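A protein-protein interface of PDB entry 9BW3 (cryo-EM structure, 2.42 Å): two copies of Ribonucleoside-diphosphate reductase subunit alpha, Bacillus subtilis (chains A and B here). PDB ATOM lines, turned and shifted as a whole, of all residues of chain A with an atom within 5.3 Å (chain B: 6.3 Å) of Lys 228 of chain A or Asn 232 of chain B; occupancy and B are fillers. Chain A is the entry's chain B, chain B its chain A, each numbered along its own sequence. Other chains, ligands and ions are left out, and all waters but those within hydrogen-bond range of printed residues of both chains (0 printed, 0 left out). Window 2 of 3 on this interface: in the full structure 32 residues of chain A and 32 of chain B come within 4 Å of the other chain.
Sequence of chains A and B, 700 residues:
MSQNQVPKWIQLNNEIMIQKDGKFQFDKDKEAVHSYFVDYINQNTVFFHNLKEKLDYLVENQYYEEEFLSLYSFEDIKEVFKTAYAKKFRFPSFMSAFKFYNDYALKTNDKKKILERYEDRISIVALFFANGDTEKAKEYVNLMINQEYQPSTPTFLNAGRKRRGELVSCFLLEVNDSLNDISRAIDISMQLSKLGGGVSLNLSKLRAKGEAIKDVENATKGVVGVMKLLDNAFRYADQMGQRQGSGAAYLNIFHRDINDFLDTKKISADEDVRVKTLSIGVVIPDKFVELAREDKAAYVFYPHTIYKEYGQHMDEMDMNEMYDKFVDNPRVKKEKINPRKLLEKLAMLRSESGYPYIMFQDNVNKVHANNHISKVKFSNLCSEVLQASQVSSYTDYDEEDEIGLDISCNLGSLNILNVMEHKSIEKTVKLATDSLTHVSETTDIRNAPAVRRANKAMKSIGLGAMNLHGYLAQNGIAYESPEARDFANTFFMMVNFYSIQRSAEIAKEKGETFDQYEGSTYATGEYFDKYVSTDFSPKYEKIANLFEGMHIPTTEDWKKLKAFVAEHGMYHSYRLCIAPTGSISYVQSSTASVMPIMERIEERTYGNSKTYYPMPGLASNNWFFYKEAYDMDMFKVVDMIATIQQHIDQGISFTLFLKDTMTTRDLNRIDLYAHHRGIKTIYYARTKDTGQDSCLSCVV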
ATOM      1  N   VAL A 223      -3.397  -2.067  11.595  1.00  0.00           N
ATOM      2  CA  VAL A 223      -4.267  -1.131  10.898  1.00  0.00           C
ATOM      3  C   VAL A 223      -3.921   0.319  11.209  1.00  0.00           C
ATOM      4  O   VAL A 223      -4.324   1.213  10.463  1.00  0.00           O
ATOM      5  CB  VAL A 223      -5.748  -1.405  11.228  1.00  0.00           C
ATOM      6  CG1 VAL A 223      -6.068  -2.880  11.060  1.00  0.00           C
ATOM      7  CG2 VAL A 223      -6.080  -0.931  12.636  1.00  0.00           C
ATOM      8  N   VAL A 224      -3.189   0.585  12.292  1.00  0.00           N
ATOM      9  CA  VAL A 224      -2.878   1.969  12.641  1.00  0.00           C
ATOM     10  C   VAL A 224      -1.847   2.573  11.690  1.00  0.00           C
ATOM     11  O   VAL A 224      -1.924   3.762  11.363  1.00  0.00           O
ATOM     12  CB  VAL A 224      -2.413   2.064  14.103  1.00  0.00           C
ATOM     13  CG1 VAL A 224      -1.924   3.469  14.409  1.00  0.00           C
ATOM     14  CG2 VAL A 224      -3.545   1.680  15.040  1.00  0.00           C
ATOM     15  N   GLY A 225      -0.868   1.789  11.235  1.00  0.00           N
ATOM     16  CA  GLY A 225       0.068   2.305  10.248  1.00  0.00           C
ATOM     17  C   GLY A 225      -0.607   2.629   8.929  1.00  0.00           C
ATOM     18  O   GLY A 225      -0.357   3.680   8.327  1.00  0.00           O
ATOM     19  N   VAL A 226      -1.482   1.735   8.465  1.00  0.00           N
ATOM     20  CA  VAL A 226      -2.264   2.017   7.269  1.00  0.00           C
ATOM     21  C   VAL A 226      -3.170   3.214   7.502  1.00  0.00           C
ATOM     22  O   VAL A 226      -3.436   3.990   6.579  1.00  0.00           O
ATOM     23  CB  VAL A 226      -3.068   0.771   6.847  1.00  0.00           C
ATOM     24  CG1 VAL A 226      -3.923   1.079   5.630  1.00  0.00           C
ATOM     25  CG2 VAL A 226      -2.130  -0.390   6.570  1.00  0.00           C
ATOM     26  N   MET A 227      -3.662   3.382   8.730  1.00  0.00           N
ATOM     27  CA  MET A 227      -4.492   4.538   9.050  1.00  0.00           C
ATOM     28  C   MET A 227      -3.699   5.832   8.933  1.00  0.00           C
ATOM     29  O   MET A 227      -4.214   6.837   8.441  1.00  0.00           O
ATOM     30  CB  MET A 227      -5.071   4.396  10.456  1.00  0.00           C
ATOM     31  CG  MET A 227      -6.360   3.604  10.527  1.00  0.00           C
ATOM     32  SD  MET A 227      -6.883   3.327  12.228  1.00  0.00           S
ATOM     33  CE  MET A 227      -7.851   4.803  12.522  1.00  0.00           C
ATOM     34  N   LYS A 228      -2.451   5.830   9.402  1.00  0.00           N
ATOM     35  CA  LYS A 228      -1.605   7.010   9.244  1.00  0.00           C
ATOM     36  C   LYS A 228      -1.334   7.293   7.773  1.00  0.00           C
ATOM     37  O   LYS A 228      -1.393   8.449   7.328  1.00  0.00           O
ATOM     38  CB  LYS A 228      -0.292   6.824  10.003  1.00  0.00           C
ATOM     39  CG  LYS A 228      -0.453   6.605  11.495  1.00  0.00           C
ATOM     40  CD  LYS A 228       0.894   6.622  12.199  1.00  0.00           C
ATOM     41  CE  LYS A 228       1.007   5.497  13.214  1.00  0.00           C
ATOM     42  NZ  LYS A 228       1.706   4.307  12.656  1.00  0.00           N
ATOM     43  N   LEU A 229      -1.040   6.244   7.001  1.00  0.00           N
ATOM     44  CA  LEU A 229      -0.861   6.412   5.562  1.00  0.00           C
ATOM     45  C   LEU A 229      -2.092   7.053   4.933  1.00  0.00           C
ATOM     46  O   LEU A 229      -1.986   8.023   4.174  1.00  0.00           O
ATOM     47  CB  LEU A 229      -0.569   5.062   4.907  1.00  0.00           C
ATOM     48  CG  LEU A 229       0.857   4.516   4.972  1.00  0.00           C
ATOM     49  CD1 LEU A 229       0.860   3.032   4.646  1.00  0.00           C
ATOM     50  CD2 LEU A 229       1.765   5.275   4.023  1.00  0.00           C
ATOM     51  N   LEU A 230      -3.274   6.520   5.246  1.00  0.00           N
ATOM     52  CA  LEU A 230      -4.512   7.021   4.659  1.00  0.00           C
ATOM     53  C   LEU A 230      -4.811   8.443   5.112  1.00  0.00           C
ATOM     54  O   LEU A 230      -5.309   9.256   4.328  1.00  0.00           O
ATOM     55  CB  LEU A 230      -5.672   6.092   5.015  1.00  0.00           C
ATOM     56  CG  LEU A 230      -5.680   4.729   4.327  1.00  0.00           C
ATOM     57  CD1 LEU A 230      -6.715   3.818   4.966  1.00  0.00           C
ATOM     58  CD2 LEU A 230      -5.940   4.885   2.839  1.00  0.00           C
ATOM     59  N   ASP A 231      -4.539   8.756   6.378  1.00  0.00           N
ATOM     60  CA  ASP A 231      -4.771  10.106   6.872  1.00  0.00           C
ATOM     61  C   ASP A 231      -3.893  11.110   6.141  1.00  0.00           C
ATOM     62  O   ASP A 231      -4.363  12.180   5.736  1.00  0.00           O
ATOM     63  CB  ASP A 231      -4.521  10.160   8.379  1.00  0.00           C
ATOM     64  CG  ASP A 231      -4.554  11.571   8.926  1.00  0.00           C
ATOM     65  OD1 ASP A 231      -5.631  12.202   8.880  1.00  0.00           O
ATOM     66  OD2 ASP A 231      -3.505  12.050   9.403  1.00  0.00           O
ATOM     67  N   ASN A 232      -2.617  10.776   5.940  1.00  0.00           N
ATOM     68  CA  ASN A 232      -1.754  11.667   5.174  1.00  0.00           C
ATOM     69  C   ASN A 232      -2.202  11.762   3.719  1.00  0.00           C
ATOM     70  O   ASN A 232      -2.125  12.834   3.110  1.00  0.00           O
ATOM     71  CB  ASN A 232      -0.301  11.210   5.264  1.00  0.00           C
ATOM     72  CG  ASN A 232       0.657  12.371   5.413  1.00  0.00           C
ATOM     73  OD1 ASN A 232       0.763  13.218   4.527  1.00  0.00           O
ATOM     74  ND2 ASN A 232       1.344  12.429   6.544  1.00  0.00           N
ATOM     75  N   ALA A 233      -2.664  10.651   3.142  1.00  0.00           N
ATOM     76  CA  ALA A 233      -3.132  10.679   1.760  1.00  0.00           C
ATOM     77  C   ALA A 233      -4.354  11.578   1.609  1.00  0.00           C
ATOM     78  O   ALA A 233      -4.468  12.326   0.632  1.00  0.00           O
ATOM     79  CB  ALA A 233      -3.444   9.261   1.284  1.00  0.00           C
ATOM     80  N   ARG A 235      -5.151  14.071   3.665  1.00  0.00           N
ATOM     81  CA  ARG A 235      -4.712  15.441   3.898  1.00  0.00           C
ATOM     82  C   ARG A 235      -4.059  16.029   2.654  1.00  0.00           C
ATOM     83  O   ARG A 235      -4.251  17.209   2.344  1.00  0.00           O
ATOM     84  CB  ARG A 235      -3.757  15.489   5.089  1.00  0.00           C
ATOM     85  CG  ARG A 235      -4.386  16.035   6.360  1.00  0.00           C
ATOM     86  CD  ARG A 235      -3.366  16.176   7.480  1.00  0.00           C
ATOM     87  NE  ARG A 235      -2.932  14.882   7.992  1.00  0.00           N
ATOM     88  CZ  ARG A 235      -1.791  14.292   7.663  1.00  0.00           C
ATOM     89  NH1 ARG A 235      -0.939  14.854   6.822  1.00  0.00           N
ATOM     90  NH2 ARG A 235      -1.496  13.109   8.194  1.00  0.00           N
ATOM     91  N   ASP A 272       2.007  10.657  16.976  1.00  0.00           N
ATOM     92  CA  ASP A 272       2.433   9.594  16.073  1.00  0.00           C
ATOM     93  C   ASP A 272       1.295   8.631  15.760  1.00  0.00           C
ATOM     94  O   ASP A 272       1.167   8.178  14.618  1.00  0.00           O
ATOM     95  CB  ASP A 272       3.623   8.840  16.669  1.00  0.00           C
ATOM     96  CG  ASP A 272       3.233   7.975  17.853  1.00  0.00           C
ATOM     97  OD1 ASP A 272       2.227   8.297  18.519  1.00  0.00           O
ATOM     98  OD2 ASP A 272       3.932   6.974  18.115  1.00  0.00           O
ATOM     99  N   VAL A 273       0.466   8.307  16.750  1.00  0.00           N
ATOM    100  CA  VAL A 273      -0.623   7.353  16.569  1.00  0.00           C
ATOM    101  C   VAL A 273      -1.909   8.089  16.222  1.00  0.00           C
ATOM    102  O   VAL A 273      -2.755   7.566  15.488  1.00  0.00           O
ATOM    103  CB  VAL A 273      -0.814   6.482  17.824  1.00  0.00           C
ATOM    104  CG1 VAL A 273      -2.223   5.912  17.859  1.00  0.00           C
ATOM    105  CG2 VAL A 273       0.214   5.364  17.851  1.00  0.00           C
ATOM    106  N   VAL A 275      -4.731  10.032  14.568  1.00  0.00           N
ATOM    107  CA  VAL A 275      -5.161  10.337  13.210  1.00  0.00           C
ATOM    108  C   VAL A 275      -6.140  11.498  13.292  1.00  0.00           C
ATOM    109  O   VAL A 275      -7.115  11.442  14.053  1.00  0.00           O
ATOM    110  CB  VAL A 275      -5.799   9.115  12.529  1.00  0.00           C
ATOM    111  CG1 VAL A 275      -6.636   9.552  11.352  1.00  0.00           C
ATOM    112  CG2 VAL A 275      -4.725   8.132  12.089  1.00  0.00           C
ATOM    113  N   MET B 190       7.583   2.186  -1.240  1.00  0.00           N
ATOM    114  CA  MET B 190       7.244   1.188  -0.230  1.00  0.00           C
ATOM    115  C   MET B 190       7.683  -0.206  -0.664  1.00  0.00           C
ATOM    116  O   MET B 190       8.185  -0.988   0.150  1.00  0.00           O
ATOM    117  CB  MET B 190       5.743   1.222   0.058  1.00  0.00           C
ATOM    118  CG  MET B 190       5.299   2.435   0.859  1.00  0.00           C
ATOM    119  SD  MET B 190       3.646   2.257   1.550  1.00  0.00           S
ATOM    120  CE  MET B 190       2.706   1.879   0.075  1.00  0.00           C
ATOM    121  N   MET B 227       6.525  15.116   0.125  1.00  0.00           N
ATOM    122  CA  MET B 227       7.550  14.666   1.060  1.00  0.00           C
ATOM    123  C   MET B 227       6.932  14.069   2.316  1.00  0.00           C
ATOM    124  O   MET B 227       7.448  13.090   2.856  1.00  0.00           O
ATOM    125  CB  MET B 227       8.486  15.817   1.421  1.00  0.00           C
ATOM    126  CG  MET B 227       9.438  16.218   0.314  1.00  0.00           C
ATOM    127  SD  MET B 227      10.136  17.851   0.593  1.00  0.00           S
ATOM    128  CE  MET B 227      11.175  17.521   2.011  1.00  0.00           C
ATOM    129  N   LYS B 228       5.843  14.658   2.812  1.00  0.00           N
ATOM    130  CA  LYS B 228       5.145  14.066   3.950  1.00  0.00           C
ATOM    131  C   LYS B 228       4.594  12.692   3.594  1.00  0.00           C
ATOM    132  O   LYS B 228       4.691  11.746   4.388  1.00  0.00           O
ATOM    133  CB  LYS B 228       4.020  14.988   4.417  1.00  0.00           C
ATOM    134  CG  LYS B 228       4.398  15.900   5.568  1.00  0.00           C
ATOM    135  CD  LYS B 228       4.420  17.352   5.124  1.00  0.00           C
ATOM    136  CE  LYS B 228       3.011  17.873   4.892  1.00  0.00           C
ATOM    137  NZ  LYS B 228       3.011  19.261   4.351  1.00  0.00           N
ATOM    138  N   LEU B 229       4.016  12.563   2.398  1.00  0.00           N
ATOM    139  CA  LEU B 229       3.535  11.259   1.950  1.00  0.00           C
ATOM    140  C   LEU B 229       4.672  10.245   1.902  1.00  0.00           C
ATOM    141  O   LEU B 229       4.530   9.108   2.365  1.00  0.00           O
ATOM    142  CB  LEU B 229       2.874  11.385   0.578  1.00  0.00           C
ATOM    143  CG  LEU B 229       1.652  12.293   0.454  1.00  0.00           C
ATOM    144  CD1 LEU B 229       1.426  12.663  -0.999  1.00  0.00           C
ATOM    145  CD2 LEU B 229       0.428  11.607   1.028  1.00  0.00           C
ATOM    146  N   LEU B 230       5.812  10.645   1.335  1.00  0.00           N
ATOM    147  CA  LEU B 230       6.958   9.748   1.225  1.00  0.00           C
ATOM    148  C   LEU B 230       7.512   9.384   2.596  1.00  0.00           C
ATOM    149  O   LEU B 230       7.918   8.242   2.823  1.00  0.00           O
ATOM    150  CB  LEU B 230       8.044  10.392   0.364  1.00  0.00           C
ATOM    151  CG  LEU B 230       7.703  10.612  -1.111  1.00  0.00           C
ATOM    152  CD1 LEU B 230       8.727  11.523  -1.769  1.00  0.00           C
ATOM    153  CD2 LEU B 230       7.613   9.284  -1.843  1.00  0.00           C
ATOM    154  N   ASP B 231       7.561  10.351   3.512  1.00  0.00           N
ATOM    155  CA  ASP B 231       8.034  10.082   4.863  1.00  0.00           C
ATOM    156  C   ASP B 231       7.142   9.067   5.560  1.00  0.00           C
ATOM    157  O   ASP B 231       7.633   8.138   6.208  1.00  0.00           O
ATOM    158  CB  ASP B 231       8.098  11.387   5.657  1.00  0.00           C
ATOM    159  CG  ASP B 231       8.675  11.200   7.044  1.00  0.00           C
ATOM    160  OD1 ASP B 231       9.916  11.169   7.171  1.00  0.00           O
ATOM    161  OD2 ASP B 231       7.890  11.088   8.007  1.00  0.00           O
ATOM    162  N   ASN B 232       5.823   9.220   5.426  1.00  0.00           N
ATOM    163  CA  ASN B 232       4.911   8.243   6.011  1.00  0.00           C
ATOM    164  C   ASN B 232       5.065   6.875   5.356  1.00  0.00           C
ATOM    165  O   ASN B 232       5.020   5.845   6.037  1.00  0.00           O
ATOM    166  CB  ASN B 232       3.472   8.737   5.903  1.00  0.00           C
ATOM    167  CG  ASN B 232       2.922   9.199   7.233  1.00  0.00           C
ATOM    168  OD1 ASN B 232       2.969  10.383   7.560  1.00  0.00           O
ATOM    169  ND2 ASN B 232       2.366   8.269   7.996  1.00  0.00           N
ATOM    170  N   ALA B 233       5.242   6.844   4.034  1.00  0.00           N
ATOM    171  CA  ALA B 233       5.419   5.571   3.342  1.00  0.00           C
ATOM    172  C   ALA B 233       6.692   4.864   3.792  1.00  0.00           C
ATOM    173  O   ALA B 233       6.694   3.645   3.998  1.00  0.00           O
ATOM    174  CB  ALA B 233       5.433   5.796   1.831  1.00  0.00           C
ATOM    175  N   PHE B 234       7.786   5.611   3.944  1.00  0.00           N
ATOM    176  CA  PHE B 234       9.041   5.013   4.386  1.00  0.00           C
ATOM    177  C   PHE B 234       8.964   4.587   5.845  1.00  0.00           C
ATOM    178  O   PHE B 234       9.568   3.583   6.238  1.00  0.00           O
ATOM    179  CB  PHE B 234      10.193   5.993   4.168  1.00  0.00           C
ATOM    180  CG  PHE B 234      10.673   6.057   2.748  1.00  0.00           C
ATOM    181  CD1 PHE B 234      11.155   4.926   2.117  1.00  0.00           C
ATOM    182  CD2 PHE B 234      10.633   7.245   2.040  1.00  0.00           C
ATOM    183  CE1 PHE B 234      11.595   4.978   0.809  1.00  0.00           C
ATOM    184  CE2 PHE B 234      11.072   7.303   0.732  1.00  0.00           C
ATOM    185  CZ  PHE B 234      11.553   6.167   0.117  1.00  0.00           C
ATOM    186  N   ARG B 235       8.229   5.341   6.663  1.00  0.00           N
ATOM    187  CA  ARG B 235       8.007   4.941   8.045  1.00  0.00           C
ATOM    188  C   ARG B 235       7.204   3.650   8.129  1.00  0.00           C
ATOM    189  O   ARG B 235       7.487   2.798   8.977  1.00  0.00           O
ATOM    190  CB  ARG B 235       7.297   6.066   8.794  1.00  0.00           C
ATOM    191  CG  ARG B 235       7.420   6.010  10.301  1.00  0.00           C
ATOM    192  CD  ARG B 235       6.211   6.655  10.964  1.00  0.00           C
ATOM    193  NE  ARG B 235       5.818   7.906  10.321  1.00  0.00           N
ATOM    194  CZ  ARG B 235       6.641   8.908  10.036  1.00  0.00           C
ATOM    195  NH1 ARG B 235       7.925   8.859  10.346  1.00  0.00           N
ATOM    196  NH2 ARG B 235       6.159   9.987   9.426  1.00  0.00           N
ATOM    197  N   TYR B 236       6.203   3.489   7.262  1.00  0.00           N
ATOM    198  CA  TYR B 236       5.387   2.281   7.290  1.00  0.00           C
ATOM    199  C   TYR B 236       6.181   1.062   6.837  1.00  0.00           C
ATOM    200  O   TYR B 236       6.117   0.003   7.470  1.00  0.00           O
ATOM    201  CB  TYR B 236       4.145   2.476   6.420  1.00  0.00           C
ATOM    202  CG  TYR B 236       3.294   1.238   6.283  1.00  0.00           C
ATOM    203  CD1 TYR B 236       2.428   0.852   7.296  1.00  0.00           C
ATOM    204  CD2 TYR B 236       3.353   0.455   5.139  1.00  0.00           C
ATOM    205  CE1 TYR B 236       1.651  -0.277   7.175  1.00  0.00           C
ATOM    206  CE2 TYR B 236       2.579  -0.675   5.009  1.00  0.00           C
ATOM    207  CZ  TYR B 236       1.728  -1.036   6.029  1.00  0.00           C
ATOM    208  OH  TYR B 236       0.954  -2.162   5.902  1.00  0.00           O
ATOM    209  N   ALA B 237       6.936   1.189   5.745  1.00  0.00           N
ATOM    210  CA  ALA B 237       7.777   0.100   5.247  1.00  0.00           C
ATOM    211  C   ALA B 237       9.130   0.178   5.949  1.00  0.00           C
ATOM    212  O   ALA B 237      10.147   0.576   5.378  1.00  0.00           O
ATOM    213  CB  ALA B 237       7.915   0.177   3.732  1.00  0.00           C
ATOM    214  N   THR B 277      11.952  10.892   8.629  1.00  0.00           N
ATOM    215  CA  THR B 277      12.650   9.739   8.077  1.00  0.00           C
ATOM    216  C   THR B 277      13.146   9.943   6.653  1.00  0.00           C
ATOM    217  O   THR B 277      13.579   8.973   6.022  1.00  0.00           O
ATOM    218  CB  THR B 277      11.744   8.503   8.122  1.00  0.00           C
ATOM    219  OG1 THR B 277      10.964   8.435   6.920  1.00  0.00           O
ATOM    220  CG2 THR B 277      10.812   8.569   9.320  1.00  0.00           C
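Tyr 236 of chain B touches Gly 225 of chain A (CD1 to C, 3.9 Å). CG2 of Val 226 of chain A touches OH of Tyr 236 of chain B, at 3.6 Å. CB of Lys 228 of chain A touches ND2 of Asn 232 of chain B, 3.6 Å away. Leu 229 of chain A touches Asn 232 of chain B. CD2 of Leu 229 of chain A touches CA of Ala 233 of chain B, 3.7 Å away. CD1 of Leu 229 of chain A touches CG of Tyr 236 of chain B (3.4 Å). Lys 228 of chain B touches Asn 232 of chain A (CB to OD1, 3.7 Å). Asn 232 of chain A touches Leu 229 of chain B (O to CD2, 3.5 Å). Leu 229 of chain B touches Ala 233 of chain A.
Of chain B, only Asn 232 (3.6 Å) comes within 4 Å of Lys 228 of chain A. Of chain A, only Lys 228, Leu 229 and Asn 232 come within 4 Å of Asn 232 of chain B. Of the printed residues of chain B, Leu 229 of chain A touches Asn 232, Ala 233 and Tyr 236. Printed residues of chain A within 4 Å of Leu 229 of chain B: Asn 232 and Ala 233. Thr 277 of chain B touches none of the printed residues of chain A. The nearest printed residue of chain A that does not touch Asn 232 of chain B is Arg 235 of chain A (5.3 Å).
OD1 of Asn 232 of chain A sits close to NH1 of Arg 235 of chain A (3.3 Å).
Hydrophobic or aromatic side chains of chain B that line the printed part of chain A: Leu 229 and Tyr 236. Of the 15 printed residues of chain A, 6 touch a printed residue of chain B. Hydrophobic or aromatic side chains of chain A within 4 Å of the printed part of chain B: Val 226 and Leu 229.
ND2 of Asn 232 of chain A lies within hydrogen-bond range of OD1 of Asn 232 of chain B, at 2.8 Å.
Lys 228 of chain A touches Asn 232 of chain B, and with the chains exchanged Asn 232 of chain A touches Lys 228 of chain B. Leu 229 of chain A touches Asn 232 of chain B, and with the chains exchanged Asn 232 of chain A touches Leu 229 of chain B. Leu 229 of chain A touches Ala 233 of chain B, and with the chains exchanged Ala 233 of chain A touches Leu 229 of chain B. Asn 232 of chain B touches its own counterpart, Asn 232 of chain A. 8 positions are printed for both chains. Of the 10 pairs that touch across the chains among the printed residues, 7 have their exchanged pair printed and touching as well.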
